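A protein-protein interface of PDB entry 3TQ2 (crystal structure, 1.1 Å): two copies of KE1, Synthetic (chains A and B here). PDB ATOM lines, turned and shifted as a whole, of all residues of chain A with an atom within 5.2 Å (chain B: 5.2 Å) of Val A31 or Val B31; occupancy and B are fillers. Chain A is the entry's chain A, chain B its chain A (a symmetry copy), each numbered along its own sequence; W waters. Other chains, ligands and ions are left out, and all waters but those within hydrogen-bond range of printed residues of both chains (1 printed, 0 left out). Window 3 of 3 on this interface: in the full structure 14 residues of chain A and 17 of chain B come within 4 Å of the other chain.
Printed residues of chain B that touch a printed residue of chain A: Leu B27, Lys B28, Val B31, Ser B32 and Lys B35.
Hydrophobic or aromatic side chains of chain B within 4 Å of the printed part of chain A: Leu B27 and Val B31.
Along chain B the printed residues that touch a printed residue of chain A span positions 27 to 35.
Among the printed residues, no Asp or Glu carboxylate lies within 4 Å of a Lys or Arg side-chain nitrogen of the other chain.
Val A31 touches just one residue of chain B: Val B31.
Printed residues of chain A within 4 Å of Val B31: Leu A27 (3.8 Å), Lys A30 (3.99 Å) and Val A31 (3.7 Å).
Printed residues of chain A within 4 Å of Leu B27: Leu A27 (3.9 Å).
Of the printed residues of chain A, Lys B28 touches Leu A27 (3.8 Å).
Of the printed residues of chain A, Lys B35 touches Lys A30 (2.8 Å) and Leu A34 (3.7 Å).
Lys A28 touches none of the printed residues of chain B.
Ser A32 touches none of the printed residues of chain B.
The nearest printed residue of chain A that does not touch Val B31 is Leu A34 (4.5 Å).
Water W1 lies within hydrogen-bond range of NZ of Lys A30 (3.0 Å), OG of Ser B32 (3.0 Å) and O of Lys B28 (3.2 Å).
Leu B27 touches its own counterpart, Leu A27.
Lys A30 touches Ser B32, but with the chains exchanged Ser A32 does not touch Lys B30 (12.0 Å).
Lys A30 touches Lys B35, but with the chains exchanged Lys A35 does not touch Lys B30 (12.3 Å).
Val B31 touches its own counterpart, Val A31.
Leu B27 touches Leu A27.
Lys B28 touches Leu A27 (N to CD2, 3.8 Å).
Val B31 touches Leu A27.
CG1 of Val B31 touches CE of Lys A30, at 3.99 Å.
Lys A30 touches Ser B32.
Val A31 touches Val B31.
Leu A34 touches Lys B35.
The backbone carbonyl oxygen (O) of Lys B28 sits at hydrogen-bond distance from the side-chain hydroxyl (OG) of Ser B32 (3.3 Å).
The side-chain amino group (NZ) of Lys A30 lies within hydrogen-bond range of the backbone carbonyl oxygen (O) of Lys B35 (2.8 Å).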
ATOM      1  N   LEU A  27      23.700  26.184   1.418  1.00  0.00           N
ATOM      2  CA  LEU A  27      23.595  26.849   2.738  1.00  0.00           C
ATOM      3  C   LEU A  27      22.551  27.951   2.700  1.00  0.00           C
ATOM      4  O   LEU A  27      21.738  28.088   3.707  1.00  0.00           O
ATOM      5  CB  LEU A  27      24.944  27.413   3.200  1.00  0.00           C
ATOM      6  CG  LEU A  27      25.053  27.853   4.680  1.00  0.00           C
ATOM      7  CD1 LEU A  27      24.657  26.778   5.667  1.00  0.00           C
ATOM      8  CD2 LEU A  27      26.485  28.303   5.004  1.00  0.00           C
ATOM      9  N   LYS A  28      22.474  28.714   1.655  1.00  0.00           N
ATOM     10  CA  LYS A  28      21.487  29.788   1.496  1.00  0.00           C
ATOM     11  C   LYS A  28      20.076  29.207   1.552  1.00  0.00           C
ATOM     12  O   LYS A  28      19.139  29.771   2.187  1.00  0.00           O
ATOM     13  CB  LYS A  28      21.739  30.511   0.154  1.00  0.00           C
ATOM     14  CG  LYS A  28      20.785  31.717   0.036  1.00  0.00           C
ATOM     15  CD  LYS A  28      21.199  32.584  -1.155  1.00  0.00           C
ATOM     16  CE  LYS A  28      20.403  33.842  -1.395  1.00  0.00           C
ATOM     17  NZ  LYS A  28      19.035  33.563  -1.926  1.00  0.00           N
ATOM     18  N   GLU A  29      19.834  28.115   0.891  1.00  0.00           N
ATOM     19  CA  GLU A  29      18.506  27.470   0.913  1.00  0.00           C
ATOM     20  C   GLU A  29      18.181  26.989   2.340  1.00  0.00           C
ATOM     21  O   GLU A  29      17.020  27.180   2.757  1.00  0.00           O
ATOM     22  CB  GLU A  29      18.437  26.347  -0.107  1.00  0.00           C
ATOM     23  CG  GLU A  29      17.064  25.648  -0.145  1.00  0.00           C
ATOM     24  CD  GLU A  29      15.868  26.526  -0.394  1.00  0.00           C
ATOM     25  OE1 GLU A  29      15.862  27.597  -1.039  1.00  0.00           O
ATOM     26  OE2 GLU A  29      14.738  26.129   0.084  1.00  0.00           O
ATOM     27  N   LYS A  30      19.152  26.393   2.983  1.00  0.00           N
ATOM     28  CA  LYS A  30      18.917  25.921   4.370  1.00  0.00           C
ATOM     29  C   LYS A  30      18.571  27.107   5.254  1.00  0.00           C
ATOM     30  O   LYS A  30      17.596  26.984   6.085  1.00  0.00           O
ATOM     31  CB  LYS A  30      20.108  25.143   4.861  1.00  0.00           C
ATOM     32  CG  LYS A  30      19.944  24.546   6.252  1.00  0.00           C
ATOM     33  CD  LYS A  30      21.061  23.590   6.622  1.00  0.00           C
ATOM     34  CE  LYS A  30      20.893  23.028   8.014  1.00  0.00           C
ATOM     35  NZ  LYS A  30      21.962  22.160   8.517  1.00  0.00           N
ATOM     36  N   VAL A  31      19.215  28.246   5.140  1.00  0.00           N
ATOM     37  CA  VAL A  31      18.966  29.427   5.958  1.00  0.00           C
ATOM     38  C   VAL A  31      17.605  29.952   5.570  1.00  0.00           C
ATOM     39  O   VAL A  31      16.871  30.372   6.510  1.00  0.00           O
ATOM     40  CB  VAL A  31      20.067  30.465   5.847  1.00  0.00           C
ATOM     41  CG1 VAL A  31      19.683  31.732   6.621  1.00  0.00           C
ATOM     42  CG2 VAL A  31      21.371  29.934   6.456  1.00  0.00           C
ATOM     43  N   SER A  32      17.173  29.938   4.338  1.00  0.00           N
ATOM     44  CA  SER A  32      15.832  30.412   3.982  1.00  0.00           C
ATOM     45  C   SER A  32      14.736  29.511   4.564  1.00  0.00           C
ATOM     46  O   SER A  32      13.641  30.089   4.804  1.00  0.00           O
ATOM     47  CB  SER A  32      15.734  30.433   2.441  1.00  0.00           C
ATOM     48  OG  SER A  32      16.413  31.598   1.943  1.00  0.00           O
ATOM     49  N   ALA A  33      15.027  28.283   4.758  1.00  0.00           N
ATOM     50  CA  ALA A  33      14.058  27.386   5.411  1.00  0.00           C
ATOM     51  C   ALA A  33      13.900  27.821   6.877  1.00  0.00           C
ATOM     52  O   ALA A  33      12.791  27.622   7.430  1.00  0.00           O
ATOM     53  CB  ALA A  33      14.447  25.947   5.299  1.00  0.00           C
ATOM     54  N   LEU A  34      14.866  28.399   7.501  1.00  0.00           N
ATOM     55  CA  LEU A  34      14.740  28.945   8.849  1.00  0.00           C
ATOM     56  C   LEU A  34      14.077  30.297   8.888  1.00  0.00           C
ATOM     57  O   LEU A  34      13.326  30.609   9.850  1.00  0.00           O
ATOM     58  CB  LEU A  34      16.116  29.042   9.547  1.00  0.00           C
ATOM     59  CG  LEU A  34      16.862  27.703   9.725  1.00  0.00           C
ATOM     60  CD1 LEU A  34      18.239  27.899  10.342  1.00  0.00           C
ATOM     61  CD2 LEU A  34      15.988  26.735  10.526  1.00  0.00           C
ATOM     62  N   LYS A  35      14.386  31.185   7.955  1.00  0.00           N
ATOM     63  CA  LYS A  35      13.937  32.549   8.025  1.00  0.00           C
ATOM     64  C   LYS A  35      13.775  33.112   6.615  1.00  0.00           C
ATOM     65  O   LYS A  35      14.764  33.105   5.858  1.00  0.00           O
ATOM     66  CB  LYS A  35      14.903  33.491   8.749  1.00  0.00           C
ATOM     67  CG  LYS A  35      14.850  34.963   8.364  1.00  0.00           C
ATOM     68  CD  LYS A  35      14.210  35.782   9.467  1.00  0.00           C
ATOM     69  CE  LYS A  35      13.285  34.943  10.335  1.00  0.00           C
ATOM     70  NZ  LYS A  35      13.489  35.245  11.788  1.00  0.00           N
ATOM     71  N   LEU B  27      30.531  29.271   8.836  1.00  0.00           N
ATOM     72  CA  LEU B  27      29.088  29.593   8.731  1.00  0.00           C
ATOM     73  C   LEU B  27      28.261  28.323   8.665  1.00  0.00           C
ATOM     74  O   LEU B  27      27.152  28.252   9.343  1.00  0.00           O
ATOM     75  CB  LEU B  27      28.791  30.484   7.518  1.00  0.00           C
ATOM     76  CG  LEU B  27      27.395  31.148   7.460  1.00  0.00           C
ATOM     77  CD1 LEU B  27      27.046  31.947   8.696  1.00  0.00           C
ATOM     78  CD2 LEU B  27      27.290  32.076   6.241  1.00  0.00           C
ATOM     79  N   LYS B  28      28.689  27.325   7.956  1.00  0.00           N
ATOM     80  CA  LYS B  28      27.989  26.039   7.845  1.00  0.00           C
ATOM     81  C   LYS B  28      27.860  25.399   9.224  1.00  0.00           C
ATOM     82  O   LYS B  28      26.796  24.832   9.607  1.00  0.00           O
ATOM     83  CB  LYS B  28      28.768  25.123   6.875  1.00  0.00           C
ATOM     84  CG  LYS B  28      27.976  23.818   6.657  1.00  0.00           C
ATOM     85  CD  LYS B  28      28.602  23.023   5.510  1.00  0.00           C
ATOM     86  CE  LYS B  28      27.924  21.733   5.121  1.00  0.00           C
ATOM     87  NZ  LYS B  28      28.125  20.652   6.132  1.00  0.00           N
ATOM     88  N   GLU B  29      28.897  25.411  10.007  1.00  0.00           N
ATOM     89  CA  GLU B  29      28.851  24.839  11.368  1.00  0.00           C
ATOM     90  C   GLU B  29      27.858  25.634  12.237  1.00  0.00           C
ATOM     91  O   GLU B  29      27.103  24.979  12.986  1.00  0.00           O
ATOM     92  CB  GLU B  29      30.241  24.788  11.976  1.00  0.00           C
ATOM     93  CG  GLU B  29      30.260  24.180  13.392  1.00  0.00           C
ATOM     94  CD  GLU B  29      29.677  22.800  13.540  1.00  0.00           C
ATOM     95  OE1 GLU B  29      29.641  21.917  12.655  1.00  0.00           O
ATOM     96  OE2 GLU B  29      29.189  22.489  14.692  1.00  0.00           O
ATOM     97  N   LYS B  30      27.913  26.937  12.131  1.00  0.00           N
ATOM     98  CA  LYS B  30      26.971  27.765  12.924  1.00  0.00           C
ATOM     99  C   LYS B  30      25.545  27.430  12.524  1.00  0.00           C
ATOM    100  O   LYS B  30      24.669  27.281  13.456  1.00  0.00           O
ATOM    101  CB  LYS B  30      27.304  29.224  12.764  1.00  0.00           C
ATOM    102  CG  LYS B  30      26.444  30.165  13.596  1.00  0.00           C
ATOM    103  CD  LYS B  30      26.948  31.595  13.582  1.00  0.00           C
ATOM    104  CE  LYS B  30      26.066  32.517  14.393  1.00  0.00           C
ATOM    105  NZ  LYS B  30      26.404  33.944  14.380  1.00  0.00           N
ATOM    106  N   VAL B  31      25.221  27.244  11.266  1.00  0.00           N
ATOM    107  CA  VAL B  31      23.877  26.940  10.789  1.00  0.00           C
ATOM    108  C   VAL B  31      23.545  25.546  11.265  1.00  0.00           C
ATOM    109  O   VAL B  31      22.365  25.356  11.677  1.00  0.00           O
ATOM    110  CB  VAL B  31      23.728  27.116   9.290  1.00  0.00           C
ATOM    111  CG1 VAL B  31      22.338  26.655   8.835  1.00  0.00           C
ATOM    112  CG2 VAL B  31      23.868  28.594   8.905  1.00  0.00           C
ATOM    113  N   SER B  32      24.431  24.588  11.300  1.00  0.00           N
ATOM    114  CA  SER B  32      24.106  23.252  11.806  1.00  0.00           C
ATOM    115  C   SER B  32      23.803  23.269  13.309  1.00  0.00           C
ATOM    116  O   SER B  32      23.010  22.371  13.705  1.00  0.00           O
ATOM    117  CB  SER B  32      25.315  22.334  11.521  1.00  0.00           C
ATOM    118  OG  SER B  32      25.298  21.950  10.136  1.00  0.00           O
ATOM    119  N   ALA B  33      24.365  24.176  14.011  1.00  0.00           N
ATOM    120  CA  ALA B  33      24.038  24.315  15.441  1.00  0.00           C
ATOM    121  C   ALA B  33      22.583  24.794  15.565  1.00  0.00           C
ATOM    122  O   ALA B  33      21.935  24.440  16.580  1.00  0.00           O
ATOM    123  CB  ALA B  33      24.983  25.226  16.156  1.00  0.00           C
ATOM    124  N   LEU B  34      22.041  25.505  14.638  1.00  0.00           N
ATOM    125  CA  LEU B  34      20.632  25.887  14.637  1.00  0.00           C
ATOM    126  C   LEU B  34      19.716  24.793  14.153  1.00  0.00           C
ATOM    127  O   LEU B  34      18.569  24.654  14.658  1.00  0.00           O
ATOM    128  CB  LEU B  34      20.393  27.153  13.784  1.00  0.00           C
ATOM    129  CG  LEU B  34      21.149  28.415  14.250  1.00  0.00           C
ATOM    130  CD1 LEU B  34      20.924  29.590  13.309  1.00  0.00           C
ATOM    131  CD2 LEU B  34      20.766  28.735  15.696  1.00  0.00           C
ATOM    132  N   LYS B  35      20.094  24.057  13.120  1.00  0.00           N
ATOM    133  CA  LYS B  35      19.205  23.119  12.488  1.00  0.00           C
ATOM    134  C   LYS B  35      20.009  21.963  11.897  1.00  0.00           C
ATOM    135  O   LYS B  35      20.896  22.225  11.062  1.00  0.00           O
ATOM    136  CB  LYS B  35      18.394  23.707  11.330  1.00  0.00           C
ATOM    137  CG  LYS B  35      17.925  22.737  10.254  1.00  0.00           C
ATOM    138  CD  LYS B  35      16.431  22.501  10.359  1.00  0.00           C
ATOM    139  CE  LYS B  35      15.912  22.760  11.765  1.00  0.00           C
ATOM    140  NZ  LYS B  35      14.636  23.542  11.733  1.00  0.00           N
HETATM  141  O   HOH W   1      24.369  23.750   7.895  1.00  0.00           O
